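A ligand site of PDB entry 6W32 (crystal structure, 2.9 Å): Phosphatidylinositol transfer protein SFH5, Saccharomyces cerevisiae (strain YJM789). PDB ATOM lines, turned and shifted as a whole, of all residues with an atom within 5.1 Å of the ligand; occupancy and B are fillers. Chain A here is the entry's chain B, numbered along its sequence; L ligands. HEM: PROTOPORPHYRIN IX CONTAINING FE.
The side-chain hydroxyl (OG) of Ser 201 sits close to a nitrogen (NA) of the ligand, at 2.8 Å. Merely in contact with the ligand: Phe 228 (3.1 Å), Val 239 (3.2 Å), Phe 221 (3.2 Å), Met 193 (3.3 Å), Phe 247 (3.3 Å), Tyr 232 (3.4 Å), Val 204 (3.4 Å), Phe 148 (3.5 Å), Ile 235 (3.5 Å), Ile 197 (3.5 Å), Val 188 (3.5 Å), Phe 208 (3.5 Å), Val 231 (3.5 Å), Ile 205 (3.7 Å), Val 224 (3.8 Å) and Phe 154 (3.8 Å). Hydrophobic or aromatic side chains within 4 Å of the ligand: Tyr 138, Phe 148, Phe 154, His 183, Tyr 185, Val 188, Met 193, Ile 197, Val 204, Ile 205, Phe 208, Phe 221, Val 224, Phe 228, Val 231, Tyr 232, Ile 235, Val 239 and Phe 247. 22 residues have an atom within 4 Å of the ligand: Tyr 138, Phe 148, Phe 154, Arg 158, His 183, Tyr 185, Val 188, Met 193, Ile 197, Ser 201, Val 204, Ile 205, Phe 208, Lys 219, Phe 221, Val 224, Phe 228, Val 231, Tyr 232, Ile 235, Val 239 and Phe 247. The nearest printed residue that does not touch the ligand is Asn 136 (4.2 Å).
The side-chain hydroxyl of Tyr 185 lies close to a ring nitrogen (ND1) of His 183, at 2.4 Å. OH of Tyr 138 sits close to NE of Arg 158 (3.5 Å). The side-chain hydroxyl (OH) of Tyr 138 lies within hydrogen-bond range of the side-chain amide nitrogen (ND2) of Asn 136 (3.4 Å). The side-chain amino group (NZ) of Lys 219 lies close to the side-chain amide nitrogen (NE2) of Gln 181 (2.9 Å). NE of Arg 158 sits close to OD1 of Asn 136, 3.4 Å away. NE2 of Gln 181 sits close to NH2 of Arg 158, at 3.2 Å. The side-chain amide oxygen (OD1) of Asn 136 is in hydrogen-bond range of a ring nitrogen (NE2) of His 183, 3.4 Å away. The backbone carbonyl oxygen of Phe 148 lies close to the side-chain sulfur of Cys 200 (3.7 Å).
An iron atom (FE) of the ligand is bound by the side-chain hydroxyl (OH) of Tyr 185 (2.3 Å). O1A of the ligand is in hydrogen-bond range of OH of Tyr 138 (2.6 Å). NZ of Lys 219 lies within salt-bridge range of O1D of the ligand (2.7 Å). The guanidinium group (NE) of Arg 158 lies within salt-bridge range of an oxygen (O2A) of the ligand. A ring nitrogen (NE2) of His 183 lies within hydrogen-bond range of an oxygen (O2A) of the ligand, 3.1 Å away.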
ATOM      1  N   ASN A 136      -2.354 -12.161  15.322  1.00  0.00           N
ATOM      2  CA  ASN A 136      -3.186 -10.985  15.127  1.00  0.00           C
ATOM      3  C   ASN A 136      -2.896  -9.994  16.248  1.00  0.00           C
ATOM      4  O   ASN A 136      -3.052 -10.329  17.428  1.00  0.00           O
ATOM      5  CB  ASN A 136      -4.666 -11.351  15.091  1.00  0.00           C
ATOM      6  CG  ASN A 136      -4.980 -12.305  13.970  1.00  0.00           C
ATOM      7  OD1 ASN A 136      -5.107 -13.520  14.188  1.00  0.00           O
ATOM      8  ND2 ASN A 136      -5.092 -11.769  12.761  1.00  0.00           N
ATOM      9  N   TYR A 138      -4.416  -7.616  17.502  1.00  0.00           N
ATOM     10  CA  TYR A 138      -5.712  -6.946  17.582  1.00  0.00           C
ATOM     11  C   TYR A 138      -5.720  -5.833  18.627  1.00  0.00           C
ATOM     12  O   TYR A 138      -6.428  -4.838  18.467  1.00  0.00           O
ATOM     13  CB  TYR A 138      -6.803  -7.975  17.867  1.00  0.00           C
ATOM     14  CG  TYR A 138      -7.206  -8.794  16.668  1.00  0.00           C
ATOM     15  CD1 TYR A 138      -7.062  -8.324  15.369  1.00  0.00           C
ATOM     16  CD2 TYR A 138      -7.743 -10.062  16.830  1.00  0.00           C
ATOM     17  CE1 TYR A 138      -7.442  -9.113  14.274  1.00  0.00           C
ATOM     18  CE2 TYR A 138      -8.135 -10.831  15.735  1.00  0.00           C
ATOM     19  CZ  TYR A 138      -7.986 -10.358  14.479  1.00  0.00           C
ATOM     20  OH  TYR A 138      -8.378 -11.164  13.451  1.00  0.00           O
ATOM     21  N   LYS A 145     -11.885   1.797  15.501  1.00  0.00           N
ATOM     22  CA  LYS A 145     -13.087   0.977  15.392  1.00  0.00           C
ATOM     23  C   LYS A 145     -13.935   1.350  14.187  1.00  0.00           C
ATOM     24  O   LYS A 145     -15.163   1.276  14.261  1.00  0.00           O
ATOM     25  CB  LYS A 145     -13.908   1.070  16.679  1.00  0.00           C
ATOM     26  CG  LYS A 145     -13.057   0.933  17.940  1.00  0.00           C
ATOM     27  CD  LYS A 145     -13.700   0.006  18.981  1.00  0.00           C
ATOM     28  CE  LYS A 145     -12.826  -0.062  20.210  1.00  0.00           C
ATOM     29  NZ  LYS A 145     -12.751  -1.422  20.817  1.00  0.00           N
ATOM     30  N   PHE A 148     -14.052  -2.150  11.757  1.00  0.00           N
ATOM     31  CA  PHE A 148     -15.037  -3.147  12.133  1.00  0.00           C
ATOM     32  C   PHE A 148     -16.431  -2.842  11.588  1.00  0.00           C
ATOM     33  O   PHE A 148     -17.293  -3.718  11.617  1.00  0.00           O
ATOM     34  CB  PHE A 148     -15.056  -3.280  13.654  1.00  0.00           C
ATOM     35  CG  PHE A 148     -13.731  -3.672  14.243  1.00  0.00           C
ATOM     36  CD1 PHE A 148     -13.009  -2.792  15.028  1.00  0.00           C
ATOM     37  CD2 PHE A 148     -13.184  -4.928  13.984  1.00  0.00           C
ATOM     38  CE1 PHE A 148     -11.763  -3.150  15.569  1.00  0.00           C
ATOM     39  CE2 PHE A 148     -11.961  -5.296  14.497  1.00  0.00           C
ATOM     40  CZ  PHE A 148     -11.240  -4.411  15.296  1.00  0.00           C
ATOM     41  N   PHE A 154     -13.173  -6.846   6.366  1.00  0.00           N
ATOM     42  CA  PHE A 154     -12.341  -7.464   7.404  1.00  0.00           C
ATOM     43  C   PHE A 154     -12.253  -8.969   7.189  1.00  0.00           C
ATOM     44  O   PHE A 154     -11.162  -9.516   7.006  1.00  0.00           O
ATOM     45  CB  PHE A 154     -12.901  -7.154   8.783  1.00  0.00           C
ATOM     46  CG  PHE A 154     -12.015  -7.593   9.894  1.00  0.00           C
ATOM     47  CD1 PHE A 154     -11.127  -6.708  10.490  1.00  0.00           C
ATOM     48  CD2 PHE A 154     -12.067  -8.903  10.377  1.00  0.00           C
ATOM     49  CE1 PHE A 154     -10.311  -7.113  11.539  1.00  0.00           C
ATOM     50  CE2 PHE A 154     -11.254  -9.310  11.404  1.00  0.00           C
ATOM     51  CZ  PHE A 154     -10.369  -8.410  11.972  1.00  0.00           C
ATOM     52  N   ARG A 158      -8.848 -11.332   6.932  1.00  0.00           N
ATOM     53  CA  ARG A 158      -8.437 -12.394   7.854  1.00  0.00           C
ATOM     54  C   ARG A 158      -8.417 -13.769   7.203  1.00  0.00           C
ATOM     55  O   ARG A 158      -7.486 -14.550   7.423  1.00  0.00           O
ATOM     56  CB  ARG A 158      -9.346 -12.427   9.078  1.00  0.00           C
ATOM     57  CG  ARG A 158      -8.955 -13.539  10.049  1.00  0.00           C
ATOM     58  CD  ARG A 158      -7.945 -13.126  11.159  1.00  0.00           C
ATOM     59  NE  ARG A 158      -7.687 -14.265  12.027  1.00  0.00           N
ATOM     60  CZ  ARG A 158      -6.789 -15.199  11.735  1.00  0.00           C
ATOM     61  NH1 ARG A 158      -6.059 -15.056  10.642  1.00  0.00           N
ATOM     62  NH2 ARG A 158      -6.600 -16.255  12.523  1.00  0.00           N
ATOM     63  N   GLN A 181      -1.922 -20.279  16.547  1.00  0.00           N
ATOM     64  CA  GLN A 181      -2.368 -18.918  16.349  1.00  0.00           C
ATOM     65  C   GLN A 181      -2.225 -18.153  17.644  1.00  0.00           C
ATOM     66  O   GLN A 181      -2.489 -18.708  18.705  1.00  0.00           O
ATOM     67  CB  GLN A 181      -3.828 -18.889  15.851  1.00  0.00           C
ATOM     68  CG  GLN A 181      -3.984 -19.476  14.451  1.00  0.00           C
ATOM     69  CD  GLN A 181      -5.426 -19.691  14.044  1.00  0.00           C
ATOM     70  OE1 GLN A 181      -5.743 -20.655  13.327  1.00  0.00           O
ATOM     71  NE2 GLN A 181      -6.308 -18.816  14.479  1.00  0.00           N
ATOM     72  N   HIS A 183      -3.362 -14.402  19.445  1.00  0.00           N
ATOM     73  CA  HIS A 183      -3.905 -13.054  19.519  1.00  0.00           C
ATOM     74  C   HIS A 183      -3.157 -12.299  20.601  1.00  0.00           C
ATOM     75  O   HIS A 183      -2.854 -12.855  21.670  1.00  0.00           O
ATOM     76  CB  HIS A 183      -5.395 -13.063  19.833  1.00  0.00           C
ATOM     77  CG  HIS A 183      -6.242 -13.546  18.712  1.00  0.00           C
ATOM     78  ND1 HIS A 183      -7.616 -13.486  18.720  1.00  0.00           N
ATOM     79  CD2 HIS A 183      -5.900 -14.118  17.523  1.00  0.00           C
ATOM     80  CE1 HIS A 183      -8.090 -13.989  17.589  1.00  0.00           C
ATOM     81  NE2 HIS A 183      -7.062 -14.393  16.859  1.00  0.00           N
ATOM     82  N   TYR A 185      -3.838  -9.072  22.583  1.00  0.00           N
ATOM     83  CA  TYR A 185      -4.792  -8.052  22.938  1.00  0.00           C
ATOM     84  C   TYR A 185      -4.185  -6.985  23.821  1.00  0.00           C
ATOM     85  O   TYR A 185      -4.918  -6.311  24.558  1.00  0.00           O
ATOM     86  CB  TYR A 185      -5.973  -8.711  23.631  1.00  0.00           C
ATOM     87  CG  TYR A 185      -6.736  -9.619  22.718  1.00  0.00           C
ATOM     88  CD1 TYR A 185      -7.406  -9.120  21.619  1.00  0.00           C
ATOM     89  CD2 TYR A 185      -6.808 -10.985  22.964  1.00  0.00           C
ATOM     90  CE1 TYR A 185      -8.111  -9.931  20.772  1.00  0.00           C
ATOM     91  CE2 TYR A 185      -7.531 -11.802  22.133  1.00  0.00           C
ATOM     92  CZ  TYR A 185      -8.188 -11.268  21.030  1.00  0.00           C
ATOM     93  OH  TYR A 185      -8.912 -12.054  20.164  1.00  0.00           O
ATOM     94  N   VAL A 188      -6.394  -3.653  25.008  1.00  0.00           N
ATOM     95  CA  VAL A 188      -7.842  -3.592  25.012  1.00  0.00           C
ATOM     96  C   VAL A 188      -8.334  -2.882  26.262  1.00  0.00           C
ATOM     97  O   VAL A 188      -7.751  -3.007  27.352  1.00  0.00           O
ATOM     98  CB  VAL A 188      -8.462  -4.995  24.902  1.00  0.00           C
ATOM     99  CG1 VAL A 188      -8.504  -5.444  23.435  1.00  0.00           C
ATOM    100  CG2 VAL A 188      -7.671  -5.976  25.755  1.00  0.00           C
ATOM    101  N   ARG A 192     -14.505  -0.601  25.673  1.00  0.00           N
ATOM    102  CA  ARG A 192     -14.638  -0.470  24.235  1.00  0.00           C
ATOM    103  C   ARG A 192     -14.864  -1.833  23.595  1.00  0.00           C
ATOM    104  O   ARG A 192     -14.073  -2.300  22.792  1.00  0.00           O
ATOM    105  CB  ARG A 192     -13.419   0.241  23.668  1.00  0.00           C
ATOM    106  CG  ARG A 192     -13.519   1.774  23.659  1.00  0.00           C
ATOM    107  CD  ARG A 192     -12.161   2.443  23.372  1.00  0.00           C
ATOM    108  NE  ARG A 192     -11.980   3.724  24.070  1.00  0.00           N
ATOM    109  CZ  ARG A 192     -11.027   3.960  24.964  1.00  0.00           C
ATOM    110  NH1 ARG A 192     -10.157   3.001  25.284  1.00  0.00           N
ATOM    111  NH2 ARG A 192     -10.934   5.157  25.544  1.00  0.00           N
ATOM    112  N   MET A 193     -15.951  -2.475  23.940  1.00  0.00           N
ATOM    113  CA  MET A 193     -16.177  -3.853  23.511  1.00  0.00           C
ATOM    114  C   MET A 193     -17.485  -3.962  22.769  1.00  0.00           C
ATOM    115  O   MET A 193     -18.284  -4.882  22.984  1.00  0.00           O
ATOM    116  CB  MET A 193     -16.138  -4.802  24.711  1.00  0.00           C
ATOM    117  CG  MET A 193     -15.797  -6.250  24.368  1.00  0.00           C
ATOM    118  SD  MET A 193     -14.068  -6.610  23.925  1.00  0.00           S
ATOM    119  CE  MET A 193     -13.234  -5.342  24.852  1.00  0.00           C
ATOM    120  N   ILE A 197     -17.144  -5.215  17.105  1.00  0.00           N
ATOM    121  CA  ILE A 197     -16.150  -6.260  17.336  1.00  0.00           C
ATOM    122  C   ILE A 197     -16.830  -7.609  17.483  1.00  0.00           C
ATOM    123  O   ILE A 197     -16.395  -8.614  16.913  1.00  0.00           O
ATOM    124  CB  ILE A 197     -15.297  -5.906  18.558  1.00  0.00           C
ATOM    125  CG1 ILE A 197     -14.350  -4.747  18.218  1.00  0.00           C
ATOM    126  CG2 ILE A 197     -14.461  -7.105  19.026  1.00  0.00           C
ATOM    127  CD1 ILE A 197     -13.842  -4.034  19.416  1.00  0.00           C
ATOM    128  N   CYS A 200     -17.572  -9.005  13.867  1.00  0.00           N
ATOM    129  CA  CYS A 200     -16.462  -9.596  13.120  1.00  0.00           C
ATOM    130  C   CYS A 200     -16.010 -10.925  13.721  1.00  0.00           C
ATOM    131  O   CYS A 200     -15.860 -11.912  12.978  1.00  0.00           O
ATOM    132  CB  CYS A 200     -15.285  -8.623  13.042  1.00  0.00           C
ATOM    133  SG  CYS A 200     -15.653  -7.016  12.297  1.00  0.00           S
ATOM    134  N   SER A 201     -15.750 -10.954  15.030  1.00  0.00           N
ATOM    135  CA  SER A 201     -15.423 -12.193  15.734  1.00  0.00           C
ATOM    136  C   SER A 201     -16.333 -13.352  15.360  1.00  0.00           C
ATOM    137  O   SER A 201     -15.876 -14.401  14.890  1.00  0.00           O
ATOM    138  CB  SER A 201     -15.508 -11.980  17.252  1.00  0.00           C
ATOM    139  OG  SER A 201     -14.241 -11.664  17.786  1.00  0.00           O
ATOM    140  N   VAL A 204     -16.008 -14.401  11.432  1.00  0.00           N
ATOM    141  CA  VAL A 204     -14.800 -15.192  11.165  1.00  0.00           C
ATOM    142  C   VAL A 204     -14.896 -16.534  11.892  1.00  0.00           C
ATOM    143  O   VAL A 204     -14.667 -17.587  11.276  1.00  0.00           O
ATOM    144  CB  VAL A 204     -13.546 -14.407  11.569  1.00  0.00           C
ATOM    145  CG1 VAL A 204     -12.315 -15.246  11.389  1.00  0.00           C
ATOM    146  CG2 VAL A 204     -13.445 -13.163  10.727  1.00  0.00           C
ATOM    147  N   ILE A 205     -15.269 -16.519  13.187  1.00  0.00           N
ATOM    148  CA  ILE A 205     -15.341 -17.776  13.945  1.00  0.00           C
ATOM    149  C   ILE A 205     -16.181 -18.812  13.211  1.00  0.00           C
ATOM    150  O   ILE A 205     -15.767 -19.978  13.070  1.00  0.00           O
ATOM    151  CB  ILE A 205     -15.875 -17.551  15.365  1.00  0.00           C
ATOM    152  CG1 ILE A 205     -14.780 -16.924  16.242  1.00  0.00           C
ATOM    153  CG2 ILE A 205     -16.190 -18.896  15.998  1.00  0.00           C
ATOM    154  CD1 ILE A 205     -15.287 -16.293  17.460  1.00  0.00           C
ATOM    155  N   PHE A 208     -14.082 -20.356  10.243  1.00  0.00           N
ATOM    156  CA  PHE A 208     -13.111 -21.307  10.808  1.00  0.00           C
ATOM    157  C   PHE A 208     -13.788 -22.589  11.270  1.00  0.00           C
ATOM    158  O   PHE A 208     -13.373 -23.696  10.888  1.00  0.00           O
ATOM    159  CB  PHE A 208     -12.343 -20.672  11.967  1.00  0.00           C
ATOM    160  CG  PHE A 208     -11.421 -19.551  11.556  1.00  0.00           C
ATOM    161  CD1 PHE A 208     -11.166 -19.264  10.217  1.00  0.00           C
ATOM    162  CD2 PHE A 208     -10.812 -18.764  12.513  1.00  0.00           C
ATOM    163  CE1 PHE A 208     -10.317 -18.222   9.854  1.00  0.00           C
ATOM    164  CE2 PHE A 208      -9.979 -17.711  12.160  1.00  0.00           C
ATOM    165  CZ  PHE A 208      -9.726 -17.436  10.841  1.00  0.00           C
ATOM    166  N   LEU A 216      -6.405 -26.375  13.496  1.00  0.00           N
ATOM    167  CA  LEU A 216      -5.794 -25.671  14.628  1.00  0.00           C
ATOM    168  C   LEU A 216      -5.235 -26.690  15.596  1.00  0.00           C
ATOM    169  O   LEU A 216      -5.897 -27.686  15.899  1.00  0.00           O
ATOM    170  CB  LEU A 216      -6.836 -24.803  15.351  1.00  0.00           C
ATOM    171  CG  LEU A 216      -6.384 -23.776  16.362  1.00  0.00           C
ATOM    172  CD1 LEU A 216      -5.675 -22.698  15.683  1.00  0.00           C
ATOM    173  CD2 LEU A 216      -7.576 -23.207  17.112  1.00  0.00           C
ATOM    174  N   LYS A 219      -4.208 -22.347  20.225  1.00  0.00           N
ATOM    175  CA  LYS A 219      -4.418 -20.913  20.059  1.00  0.00           C
ATOM    176  C   LYS A 219      -4.188 -20.210  21.412  1.00  0.00           C
ATOM    177  O   LYS A 219      -4.753 -20.628  22.435  1.00  0.00           O
ATOM    178  CB  LYS A 219      -5.808 -20.653  19.508  1.00  0.00           C
ATOM    179  CG  LYS A 219      -6.088 -19.206  19.137  1.00  0.00           C
ATOM    180  CD  LYS A 219      -7.106 -19.124  18.016  1.00  0.00           C
ATOM    181  CE  LYS A 219      -7.158 -17.759  17.356  1.00  0.00           C
ATOM    182  NZ  LYS A 219      -8.277 -17.694  16.349  1.00  0.00           N
ATOM    183  N   PHE A 221      -4.068 -16.581  23.658  1.00  0.00           N
ATOM    184  CA  PHE A 221      -4.683 -15.263  23.762  1.00  0.00           C
ATOM    185  C   PHE A 221      -3.902 -14.540  24.844  1.00  0.00           C
ATOM    186  O   PHE A 221      -4.155 -14.762  26.022  1.00  0.00           O
ATOM    187  CB  PHE A 221      -6.153 -15.375  24.146  1.00  0.00           C
ATOM    188  CG  PHE A 221      -6.966 -16.166  23.179  1.00  0.00           C
ATOM    189  CD1 PHE A 221      -7.720 -15.534  22.216  1.00  0.00           C
ATOM    190  CD2 PHE A 221      -6.966 -17.550  23.232  1.00  0.00           C
ATOM    191  CE1 PHE A 221      -8.503 -16.258  21.316  1.00  0.00           C
ATOM    192  CE2 PHE A 221      -7.729 -18.287  22.331  1.00  0.00           C
ATOM    193  CZ  PHE A 221      -8.516 -17.623  21.369  1.00  0.00           C
ATOM    194  N   VAL A 224      -4.124 -10.302  28.213  1.00  0.00           N
ATOM    195  CA  VAL A 224      -5.562 -10.218  28.480  1.00  0.00           C
ATOM    196  C   VAL A 224      -5.757 -10.045  29.984  1.00  0.00           C
ATOM    197  O   VAL A 224      -5.595 -11.012  30.744  1.00  0.00           O
ATOM    198  CB  VAL A 224      -6.287 -11.488  28.005  1.00  0.00           C
ATOM    199  CG1 VAL A 224      -7.797 -11.287  27.969  1.00  0.00           C
ATOM    200  CG2 VAL A 224      -5.760 -11.957  26.675  1.00  0.00           C
ATOM    201  N   PHE A 228     -11.660  -9.389  31.878  1.00  0.00           N
ATOM    202  CA  PHE A 228     -12.160  -9.772  30.573  1.00  0.00           C
ATOM    203  C   PHE A 228     -12.787 -11.151  30.575  1.00  0.00           C
ATOM    204  O   PHE A 228     -13.093 -11.695  29.498  1.00  0.00           O
ATOM    205  CB  PHE A 228     -11.010  -9.715  29.565  1.00  0.00           C
ATOM    206  CG  PHE A 228     -10.792  -8.356  28.975  1.00  0.00           C
ATOM    207  CD1 PHE A 228     -11.654  -7.853  28.023  1.00  0.00           C
ATOM    208  CD2 PHE A 228      -9.726  -7.576  29.385  1.00  0.00           C
ATOM    209  CE1 PHE A 228     -11.468  -6.612  27.497  1.00  0.00           C
ATOM    210  CE2 PHE A 228      -9.539  -6.323  28.840  1.00  0.00           C
ATOM    211  CZ  PHE A 228     -10.411  -5.836  27.909  1.00  0.00           C
ATOM    212  N   VAL A 231     -15.957 -11.559  28.551  1.00  0.00           N
ATOM    213  CA  VAL A 231     -15.765 -11.633  27.116  1.00  0.00           C
ATOM    214  C   VAL A 231     -15.441 -13.071  26.716  1.00  0.00           C
ATOM    215  O   VAL A 231     -16.121 -13.674  25.883  1.00  0.00           O
ATOM    216  CB  VAL A 231     -14.662 -10.671  26.669  1.00  0.00           C
ATOM    217  CG1 VAL A 231     -14.260 -10.951  25.193  1.00  0.00           C
ATOM    218  CG2 VAL A 231     -15.094  -9.230  26.888  1.00  0.00           C
ATOM    219  N   TYR A 232     -14.397 -13.633  27.337  1.00  0.00           N
ATOM    220  CA  TYR A 232     -13.973 -14.985  26.994  1.00  0.00           C
ATOM    221  C   TYR A 232     -15.101 -15.991  27.154  1.00  0.00           C
ATOM    222  O   TYR A 232     -15.230 -16.930  26.370  1.00  0.00           O
ATOM    223  CB  TYR A 232     -12.799 -15.399  27.861  1.00  0.00           C
ATOM    224  CG  TYR A 232     -12.119 -16.692  27.480  1.00  0.00           C
ATOM    225  CD1 TYR A 232     -11.497 -16.834  26.245  1.00  0.00           C
ATOM    226  CD2 TYR A 232     -12.039 -17.749  28.390  1.00  0.00           C
ATOM    227  CE1 TYR A 232     -10.844 -18.016  25.911  1.00  0.00           C
ATOM    228  CE2 TYR A 232     -11.399 -18.945  28.069  1.00  0.00           C
ATOM    229  CZ  TYR A 232     -10.801 -19.070  26.826  1.00  0.00           C
ATOM    230  OH  TYR A 232     -10.137 -20.245  26.513  1.00  0.00           O
ATOM    231  N   ILE A 235     -17.677 -15.359  24.089  1.00  0.00           N
ATOM    232  CA  ILE A 235     -17.199 -15.753  22.759  1.00  0.00           C
ATOM    233  C   ILE A 235     -17.165 -17.276  22.639  1.00  0.00           C
ATOM    234  O   ILE A 235     -17.677 -17.846  21.659  1.00  0.00           O
ATOM    235  CB  ILE A 235     -15.824 -15.132  22.460  1.00  0.00           C
ATOM    236  CG1 ILE A 235     -15.950 -13.611  22.334  1.00  0.00           C
ATOM    237  CG2 ILE A 235     -15.264 -15.729  21.187  1.00  0.00           C
ATOM    238  CD1 ILE A 235     -14.819 -12.948  21.516  1.00  0.00           C
ATOM    239  N   LYS A 236     -16.589 -17.959  23.634  1.00  0.00           N
ATOM    240  CA  LYS A 236     -16.434 -19.419  23.610  1.00  0.00           C
ATOM    241  C   LYS A 236     -17.723 -20.152  23.261  1.00  0.00           C
ATOM    242  O   LYS A 236     -17.670 -21.287  22.778  1.00  0.00           O
ATOM    243  CB  LYS A 236     -15.976 -19.926  24.972  1.00  0.00           C
ATOM    244  CG  LYS A 236     -14.492 -19.882  25.203  1.00  0.00           C
ATOM    245  CD  LYS A 236     -14.091 -20.666  26.460  1.00  0.00           C
ATOM    246  CE  LYS A 236     -15.069 -20.457  27.567  1.00  0.00           C
ATOM    247  NZ  LYS A 236     -14.333 -20.519  28.854  1.00  0.00           N
ATOM    248  N   VAL A 239     -17.744 -21.652  19.670  1.00  0.00           N
ATOM    249  CA  VAL A 239     -16.830 -22.672  19.162  1.00  0.00           C
ATOM    250  C   VAL A 239     -17.138 -24.007  19.807  1.00  0.00           C
ATOM    251  O   VAL A 239     -17.681 -24.076  20.928  1.00  0.00           O
ATOM    252  CB  VAL A 239     -15.339 -22.330  19.366  1.00  0.00           C
ATOM    253  CG1 VAL A 239     -14.989 -21.106  18.621  1.00  0.00           C
ATOM    254  CG2 VAL A 239     -15.057 -22.088  20.825  1.00  0.00           C
ATOM    255  N   PHE A 247      -7.631 -23.820  23.477  1.00  0.00           N
ATOM    256  CA  PHE A 247      -7.505 -22.428  23.873  1.00  0.00           C
ATOM    257  C   PHE A 247      -6.729 -22.245  25.192  1.00  0.00           C
ATOM    258  O   PHE A 247      -7.011 -22.928  26.171  1.00  0.00           O
ATOM    259  CB  PHE A 247      -8.901 -21.822  24.040  1.00  0.00           C
ATOM    260  CG  PHE A 247      -9.586 -21.578  22.749  1.00  0.00           C
ATOM    261  CD1 PHE A 247      -8.967 -21.876  21.541  1.00  0.00           C
ATOM    262  CD2 PHE A 247     -10.844 -20.980  22.722  1.00  0.00           C
ATOM    263  CE1 PHE A 247      -9.591 -21.625  20.341  1.00  0.00           C
ATOM    264  CE2 PHE A 247     -11.469 -20.746  21.528  1.00  0.00           C
ATOM    265  CZ  PHE A 247     -10.831 -21.068  20.338  1.00  0.00           C
ATOM    266  N   VAL A 249      -5.282 -18.833  27.668  1.00  0.00           N
ATOM    267  CA  VAL A 249      -5.377 -17.402  27.917  1.00  0.00           C
ATOM    268  C   VAL A 249      -4.242 -16.989  28.853  1.00  0.00           C
ATOM    269  O   VAL A 249      -4.087 -17.571  29.939  1.00  0.00           O
ATOM    270  CB  VAL A 249      -6.735 -17.042  28.540  1.00  0.00           C
ATOM    271  CG1 VAL A 249      -6.905 -15.564  28.676  1.00  0.00           C
ATOM    272  CG2 VAL A 249      -7.845 -17.646  27.721  1.00  0.00           C
HETATM  273  CHA HEM L   1     -11.902 -14.559  18.377  1.00  0.00           C
HETATM  274  CHB HEM L   1     -11.233  -9.881  17.538  1.00  0.00           C
HETATM  275  CHC HEM L   1     -10.933  -9.112  22.307  1.00  0.00           C
HETATM  276  CHD HEM L   1     -11.106 -13.911  23.120  1.00  0.00           C
HETATM  277  C1A HEM L   1     -11.735 -13.352  17.757  1.00  0.00           C
HETATM  278  C2A HEM L   1     -11.849 -13.171  16.339  1.00  0.00           C
HETATM  279  C3A HEM L   1     -11.707 -11.861  16.079  1.00  0.00           C
HETATM  280  C4A HEM L   1     -11.461 -11.206  17.353  1.00  0.00           C
HETATM  281  CMA HEM L   1     -11.722 -11.084  14.733  1.00  0.00           C
HETATM  282  CAA HEM L   1     -12.191 -14.386  15.457  1.00  0.00           C
HETATM  283  CBA HEM L   1     -11.106 -14.972  14.586  1.00  0.00           C
HETATM  284  CGA HEM L   1      -9.730 -14.444  14.753  1.00  0.00           C
HETATM  285  O1A HEM L   1      -9.584 -13.282  14.261  1.00  0.00           O
HETATM  286  O2A HEM L   1      -8.874 -15.362  14.551  1.00  0.00           O
HETATM  287  C1B HEM L   1     -11.156  -9.261  18.755  1.00  0.00           C
HETATM  288  C2B HEM L   1     -11.055  -7.837  18.934  1.00  0.00           C
HETATM  289  C3B HEM L   1     -10.969  -7.611  20.252  1.00  0.00           C
HETATM  290  C4B HEM L   1     -11.013  -8.893  20.944  1.00  0.00           C
HETATM  291  CMB HEM L   1     -11.042  -6.828  17.767  1.00  0.00           C
HETATM  292  CAB HEM L   1     -10.819  -6.233  20.927  1.00  0.00           C
HETATM  293  CBB HEM L   1     -11.621  -5.847  21.910  1.00  0.00           C
HETATM  294  C1C HEM L   1     -10.931 -10.322  22.982  1.00  0.00           C
HETATM  295  C2C HEM L   1     -10.824 -10.576  24.435  1.00  0.00           C
HETATM  296  C3C HEM L   1     -10.878 -11.904  24.653  1.00  0.00           C
HETATM  297  C4C HEM L   1     -11.012 -12.555  23.346  1.00  0.00           C
HETATM  298  CMC HEM L   1     -10.664  -9.498  25.546  1.00  0.00           C
HETATM  299  CAC HEM L   1     -10.790 -12.639  26.018  1.00  0.00           C
HETATM  300  CBC HEM L   1     -10.037 -13.760  26.173  1.00  0.00           C
HETATM  301  C1D HEM L   1     -11.386 -14.545  21.935  1.00  0.00           C
HETATM  302  C2D HEM L   1     -11.671 -15.949  21.745  1.00  0.00           C
HETATM  303  C3D HEM L   1     -11.942 -16.105  20.255  1.00  0.00           C
HETATM  304  C4D HEM L   1     -11.787 -14.804  19.705  1.00  0.00           C
HETATM  305  CMD HEM L   1     -11.693 -17.072  22.788  1.00  0.00           C
HETATM  306  CAD HEM L   1     -12.257 -17.351  19.409  1.00  0.00           C
HETATM  307  CBD HEM L   1     -11.002 -17.645  18.590  1.00  0.00           C
HETATM  308  CGD HEM L   1     -11.224 -18.937  17.827  1.00  0.00           C
HETATM  309  O1D HEM L   1     -10.359 -19.277  16.958  1.00  0.00           O
HETATM  310  O2D HEM L   1     -12.390 -19.461  17.904  1.00  0.00           O
HETATM  311  NA  HEM L   1     -11.520 -12.134  18.351  1.00  0.00           N
HETATM  312  NB  HEM L   1     -11.125  -9.869  19.994  1.00  0.00           N
HETATM  313  NC  HEM L   1     -11.046 -11.538  22.415  1.00  0.00           N
HETATM  314  ND  HEM L   1     -11.494 -13.891  20.697  1.00  0.00           N
HETATM  315 FE   HEM L   1     -11.188 -11.868  20.363  1.00  0.00          FE
